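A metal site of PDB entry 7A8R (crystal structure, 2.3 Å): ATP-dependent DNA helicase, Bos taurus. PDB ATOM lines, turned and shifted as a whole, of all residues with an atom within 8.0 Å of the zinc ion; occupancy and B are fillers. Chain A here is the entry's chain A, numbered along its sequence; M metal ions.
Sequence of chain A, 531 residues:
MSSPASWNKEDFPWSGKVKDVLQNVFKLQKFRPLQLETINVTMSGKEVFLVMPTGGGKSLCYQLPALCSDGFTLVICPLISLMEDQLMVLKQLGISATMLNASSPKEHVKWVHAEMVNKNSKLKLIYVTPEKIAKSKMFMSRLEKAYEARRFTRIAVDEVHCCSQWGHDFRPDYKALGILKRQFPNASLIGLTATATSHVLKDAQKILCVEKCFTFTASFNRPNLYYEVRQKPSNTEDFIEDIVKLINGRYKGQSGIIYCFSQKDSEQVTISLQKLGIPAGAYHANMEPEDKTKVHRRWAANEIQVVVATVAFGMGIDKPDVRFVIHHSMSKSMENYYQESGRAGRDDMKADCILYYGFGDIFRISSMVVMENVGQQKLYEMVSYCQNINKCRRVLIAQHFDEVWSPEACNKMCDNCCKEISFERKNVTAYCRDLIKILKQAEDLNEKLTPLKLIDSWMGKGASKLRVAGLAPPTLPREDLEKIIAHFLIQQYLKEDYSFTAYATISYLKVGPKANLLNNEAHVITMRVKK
The zinc ion is bound by SG of Cys 417 (2.3 Å), SG of Cys 414 (2.3 Å), SG of Cys 410 (2.3 Å) and SG of Cys 392 (2.3 Å).
Within 4 Å of the zinc ion: Cys 392, Cys 410, Cys 414 and Cys 417. The nearest printed residue that does not touch the zinc ion is Arg 393 (4.1 Å).
The side-chain sulfur of Cys 414 sits close to the backbone NH of Arg 393, at 3.4 Å. The side-chain sulfur (SG) of Cys 414 sits close to the backbone NH (N) of Asn 416 (3.8 Å). The side-chain sulfur of Cys 418 is in hydrogen-bond range of the backbone carbonyl oxygen of Cys 414, at 3.3 Å. The guanidinium group of Arg 394 lies close to the side-chain sulfur of Cys 410. The side-chain sulfur (SG) of Cys 410 lies close to the backbone NH (N) of Met 413 (3.3 Å). N of Arg 394 sits close to SG of Cys 392 (3.3 Å). N of Val 395 sits close to SG of Cys 392, at 3.7 Å.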
ATOM      1  N   LEU A 225       1.766  -7.348  12.799  1.00  0.00           N
ATOM      2  CA  LEU A 225       2.191  -7.130  14.181  1.00  0.00           C
ATOM      3  C   LEU A 225       2.100  -8.433  14.970  1.00  0.00           C
ATOM      4  O   LEU A 225       1.111  -9.156  14.884  1.00  0.00           O
ATOM      5  CB  LEU A 225       1.325  -6.055  14.843  1.00  0.00           C
ATOM      6  CG  LEU A 225       1.476  -4.642  14.292  1.00  0.00           C
ATOM      7  CD1 LEU A 225       0.736  -3.668  15.178  1.00  0.00           C
ATOM      8  CD2 LEU A 225       2.938  -4.261  14.197  1.00  0.00           C
ATOM      9  N   TYR A 226       3.162  -8.736  15.723  1.00  0.00           N
ATOM     10  CA  TYR A 226       3.227  -9.902  16.586  1.00  0.00           C
ATOM     11  C   TYR A 226       2.971  -9.460  18.034  1.00  0.00           C
ATOM     12  O   TYR A 226       3.735  -8.657  18.573  1.00  0.00           O
ATOM     13  CB  TYR A 226       4.606 -10.579  16.465  1.00  0.00           C
ATOM     14  CG  TYR A 226       4.817 -11.774  17.370  1.00  0.00           C
ATOM     15  CD1 TYR A 226       5.356 -11.630  18.646  1.00  0.00           C
ATOM     16  CD2 TYR A 226       4.481 -13.057  16.950  1.00  0.00           C
ATOM     17  CE1 TYR A 226       5.554 -12.728  19.488  1.00  0.00           C
ATOM     18  CE2 TYR A 226       4.663 -14.161  17.782  1.00  0.00           C
ATOM     19  CZ  TYR A 226       5.202 -13.988  19.044  1.00  0.00           C
ATOM     20  OH  TYR A 226       5.402 -15.079  19.881  1.00  0.00           O
ATOM     21  N   TYR A 227       1.911  -9.994  18.650  1.00  0.00           N
ATOM     22  CA  TYR A 227       1.561  -9.614  20.008  1.00  0.00           C
ATOM     23  C   TYR A 227       2.061 -10.661  20.992  1.00  0.00           C
ATOM     24  O   TYR A 227       1.836 -11.864  20.806  1.00  0.00           O
ATOM     25  CB  TYR A 227       0.040  -9.456  20.153  1.00  0.00           C
ATOM     26  CG  TYR A 227      -0.539  -8.337  19.316  1.00  0.00           C
ATOM     27  CD1 TYR A 227      -0.336  -7.007  19.670  1.00  0.00           C
ATOM     28  CD2 TYR A 227      -1.287  -8.616  18.180  1.00  0.00           C
ATOM     29  CE1 TYR A 227      -0.877  -5.969  18.906  1.00  0.00           C
ATOM     30  CE2 TYR A 227      -1.830  -7.587  17.405  1.00  0.00           C
ATOM     31  CZ  TYR A 227      -1.613  -6.259  17.776  1.00  0.00           C
ATOM     32  OH  TYR A 227      -2.148  -5.227  17.024  1.00  0.00           O
ATOM     33  N   LYS A 391      -6.310 -18.248  24.323  1.00  0.00           N
ATOM     34  CA  LYS A 391      -6.943 -17.571  23.194  1.00  0.00           C
ATOM     35  C   LYS A 391      -5.930 -16.757  22.392  1.00  0.00           C
ATOM     36  O   LYS A 391      -4.929 -16.268  22.940  1.00  0.00           O
ATOM     37  CB  LYS A 391      -8.075 -16.644  23.639  1.00  0.00           C
ATOM     38  CG  LYS A 391      -9.451 -17.305  23.671  1.00  0.00           C
ATOM     39  CD  LYS A 391     -10.566 -16.260  23.682  1.00  0.00           C
ATOM     40  CE  LYS A 391     -11.839 -16.804  24.316  1.00  0.00           C
ATOM     41  NZ  LYS A 391     -11.681 -17.051  25.784  1.00  0.00           N
ATOM     42  N   CYS A 392      -6.203 -16.617  21.097  1.00  0.00           N
ATOM     43  CA  CYS A 392      -5.410 -15.752  20.241  1.00  0.00           C
ATOM     44  C   CYS A 392      -5.472 -14.309  20.734  1.00  0.00           C
ATOM     45  O   CYS A 392      -6.555 -13.754  20.941  1.00  0.00           O
ATOM     46  CB  CYS A 392      -5.906 -15.846  18.795  1.00  0.00           C
ATOM     47  SG  CYS A 392      -5.215 -14.602  17.696  1.00  0.00           S
ATOM     48  N   ARG A 393      -4.300 -13.697  20.935  1.00  0.00           N
ATOM     49  CA  ARG A 393      -4.268 -12.316  21.414  1.00  0.00           C
ATOM     50  C   ARG A 393      -4.989 -11.368  20.481  1.00  0.00           C
ATOM     51  O   ARG A 393      -5.540 -10.351  20.926  1.00  0.00           O
ATOM     52  CB  ARG A 393      -2.820 -11.859  21.622  1.00  0.00           C
ATOM     53  CG  ARG A 393      -2.040 -12.775  22.530  1.00  0.00           C
ATOM     54  CD  ARG A 393      -1.337 -12.024  23.639  1.00  0.00           C
ATOM     55  NE  ARG A 393      -0.725 -12.943  24.605  1.00  0.00           N
ATOM     56  CZ  ARG A 393      -1.228 -13.197  25.809  1.00  0.00           C
ATOM     57  NH1 ARG A 393      -2.336 -12.590  26.204  1.00  0.00           N
ATOM     58  NH2 ARG A 393      -0.613 -14.048  26.633  1.00  0.00           N
ATOM     59  N   ARG A 394      -4.990 -11.664  19.183  1.00  0.00           N
ATOM     60  CA  ARG A 394      -5.680 -10.797  18.225  1.00  0.00           C
ATOM     61  C   ARG A 394      -7.191 -10.871  18.410  1.00  0.00           C
ATOM     62  O   ARG A 394      -7.894  -9.876  18.243  1.00  0.00           O
ATOM     63  CB  ARG A 394      -5.279 -11.209  16.810  1.00  0.00           C
ATOM     64  CG  ARG A 394      -5.493 -10.186  15.722  1.00  0.00           C
ATOM     65  CD  ARG A 394      -4.781 -10.633  14.459  1.00  0.00           C
ATOM     66  NE  ARG A 394      -3.402 -10.996  14.763  1.00  0.00           N
ATOM     67  CZ  ARG A 394      -2.351 -10.210  14.540  1.00  0.00           C
ATOM     68  NH1 ARG A 394      -2.506  -9.012  13.999  1.00  0.00           N
ATOM     69  NH2 ARG A 394      -1.138 -10.629  14.869  1.00  0.00           N
ATOM     70  N   VAL A 395      -7.700 -12.052  18.766  1.00  0.00           N
ATOM     71  CA  VAL A 395      -9.122 -12.205  19.058  1.00  0.00           C
ATOM     72  C   VAL A 395      -9.512 -11.364  20.262  1.00  0.00           C
ATOM     73  O   VAL A 395     -10.570 -10.716  20.269  1.00  0.00           O
ATOM     74  CB  VAL A 395      -9.457 -13.696  19.261  1.00  0.00           C
ATOM     75  CG1 VAL A 395     -10.790 -13.855  19.981  1.00  0.00           C
ATOM     76  CG2 VAL A 395      -9.479 -14.413  17.919  1.00  0.00           C
ATOM     77  N   LEU A 396      -8.667 -11.349  21.295  1.00  0.00           N
ATOM     78  CA  LEU A 396      -8.982 -10.618  22.516  1.00  0.00           C
ATOM     79  C   LEU A 396      -9.014  -9.112  22.266  1.00  0.00           C
ATOM     80  O   LEU A 396      -9.895  -8.403  22.778  1.00  0.00           O
ATOM     81  CB  LEU A 396      -7.955 -10.960  23.599  1.00  0.00           C
ATOM     82  CG  LEU A 396      -7.771 -12.441  23.911  1.00  0.00           C
ATOM     83  CD1 LEU A 396      -6.551 -12.654  24.791  1.00  0.00           C
ATOM     84  CD2 LEU A 396      -9.013 -13.004  24.563  1.00  0.00           C
ATOM     85  N   ALA A 409      -7.585 -14.038   9.824  1.00  0.00           N
ATOM     86  CA  ALA A 409      -6.836 -14.998  10.637  1.00  0.00           C
ATOM     87  C   ALA A 409      -5.484 -14.476  11.107  1.00  0.00           C
ATOM     88  O   ALA A 409      -4.759 -13.795  10.375  1.00  0.00           O
ATOM     89  CB  ALA A 409      -6.634 -16.295   9.847  1.00  0.00           C
ATOM     90  N   CYS A 410      -5.137 -14.825  12.360  1.00  0.00           N
ATOM     91  CA  CYS A 410      -3.879 -14.413  12.957  1.00  0.00           C
ATOM     92  C   CYS A 410      -2.675 -15.030  12.238  1.00  0.00           C
ATOM     93  O   CYS A 410      -1.686 -14.353  11.974  1.00  0.00           O
ATOM     94  CB  CYS A 410      -3.869 -14.792  14.443  1.00  0.00           C
ATOM     95  SG  CYS A 410      -2.365 -14.375  15.352  1.00  0.00           S
ATOM     96  N   ASN A 411      -2.747 -16.326  11.935  1.00  0.00           N
ATOM     97  CA  ASN A 411      -1.670 -17.045  11.244  1.00  0.00           C
ATOM     98  C   ASN A 411      -0.361 -16.985  12.037  1.00  0.00           C
ATOM     99  O   ASN A 411       0.666 -16.522  11.551  1.00  0.00           O
ATOM    100  CB  ASN A 411      -1.471 -16.521   9.827  1.00  0.00           C
ATOM    101  CG  ASN A 411      -2.488 -17.064   8.848  1.00  0.00           C
ATOM    102  OD1 ASN A 411      -3.253 -16.312   8.259  1.00  0.00           O
ATOM    103  ND2 ASN A 411      -2.500 -18.381   8.684  1.00  0.00           N
ATOM    104  N   LYS A 412      -0.425 -17.501  13.263  1.00  0.00           N
ATOM    105  CA  LYS A 412       0.732 -17.585  14.155  1.00  0.00           C
ATOM    106  C   LYS A 412       1.489 -16.260  14.237  1.00  0.00           C
ATOM    107  O   LYS A 412       2.695 -16.189  14.001  1.00  0.00           O
ATOM    108  CB  LYS A 412       1.668 -18.725  13.710  1.00  0.00           C
ATOM    109  CG  LYS A 412       1.040 -20.111  13.723  1.00  0.00           C
ATOM    110  CD  LYS A 412       2.067 -21.172  14.089  1.00  0.00           C
ATOM    111  CE  LYS A 412       2.303 -22.166  12.956  1.00  0.00           C
ATOM    112  NZ  LYS A 412       1.678 -23.502  13.227  1.00  0.00           N
ATOM    113  N   MET A 413       0.760 -15.203  14.594  1.00  0.00           N
ATOM    114  CA  MET A 413       1.327 -13.876  14.814  1.00  0.00           C
ATOM    115  C   MET A 413       0.968 -13.349  16.206  1.00  0.00           C
ATOM    116  O   MET A 413       0.726 -12.150  16.388  1.00  0.00           O
ATOM    117  CB  MET A 413       0.870 -12.894  13.729  1.00  0.00           C
ATOM    118  CG  MET A 413       1.596 -13.045  12.400  1.00  0.00           C
ATOM    119  SD  MET A 413       3.361 -12.691  12.496  1.00  0.00           S
ATOM    120  CE  MET A 413       3.358 -10.903  12.592  1.00  0.00           C
ATOM    121  N   CYS A 414       0.893 -14.248  17.179  1.00  0.00           N
ATOM    122  CA  CYS A 414       0.822 -13.887  18.584  1.00  0.00           C
ATOM    123  C   CYS A 414       1.377 -15.075  19.361  1.00  0.00           C
ATOM    124  O   CYS A 414       1.469 -16.186  18.834  1.00  0.00           O
ATOM    125  CB  CYS A 414      -0.603 -13.533  19.021  1.00  0.00           C
ATOM    126  SG  CYS A 414      -1.701 -14.932  19.197  1.00  0.00           S
ATOM    127  N   ASP A 415       1.800 -14.813  20.602  1.00  0.00           N
ATOM    128  CA  ASP A 415       2.486 -15.852  21.378  1.00  0.00           C
ATOM    129  C   ASP A 415       1.572 -17.028  21.677  1.00  0.00           C
ATOM    130  O   ASP A 415       2.028 -18.176  21.724  1.00  0.00           O
ATOM    131  CB  ASP A 415       3.078 -15.279  22.668  1.00  0.00           C
ATOM    132  CG  ASP A 415       2.057 -14.623  23.558  1.00  0.00           C
ATOM    133  OD1 ASP A 415       0.889 -14.448  23.118  1.00  0.00           O
ATOM    134  OD2 ASP A 415       2.426 -14.285  24.698  1.00  0.00           O
ATOM    135  N   ASN A 416       0.271 -16.775  21.863  1.00  0.00           N
ATOM    136  CA  ASN A 416      -0.648 -17.848  22.209  1.00  0.00           C
ATOM    137  C   ASN A 416      -0.924 -18.765  21.027  1.00  0.00           C
ATOM    138  O   ASN A 416      -1.254 -19.937  21.238  1.00  0.00           O
ATOM    139  CB  ASN A 416      -1.947 -17.274  22.763  1.00  0.00           C
ATOM    140  CG  ASN A 416      -1.808 -16.791  24.191  1.00  0.00           C
ATOM    141  OD1 ASN A 416      -0.873 -17.171  24.889  1.00  0.00           O
ATOM    142  ND2 ASN A 416      -2.736 -15.952  24.639  1.00  0.00           N
ATOM    143  N   CYS A 417      -0.772 -18.276  19.796  1.00  0.00           N
ATOM    144  CA  CYS A 417      -0.938 -19.131  18.628  1.00  0.00           C
ATOM    145  C   CYS A 417       0.337 -19.886  18.280  1.00  0.00           C
ATOM    146  O   CYS A 417       0.254 -20.915  17.606  1.00  0.00           O
ATOM    147  CB  CYS A 417      -1.380 -18.299  17.411  1.00  0.00           C
ATOM    148  SG  CYS A 417      -3.081 -17.632  17.417  1.00  0.00           S
ATOM    149  N   CYS A 418       1.495 -19.414  18.742  1.00  0.00           N
ATOM    150  CA  CYS A 418       2.791 -20.021  18.439  1.00  0.00           C
ATOM    151  C   CYS A 418       3.272 -20.996  19.506  1.00  0.00           C
ATOM    152  O   CYS A 418       3.931 -21.983  19.181  1.00  0.00           O
ATOM    153  CB  CYS A 418       3.855 -18.944  18.225  1.00  0.00           C
ATOM    154  SG  CYS A 418       3.562 -17.841  16.822  1.00  0.00           S
HETATM  155 ZN    ZN M   1      -3.038 -15.328  17.356  1.00  0.00          ZN
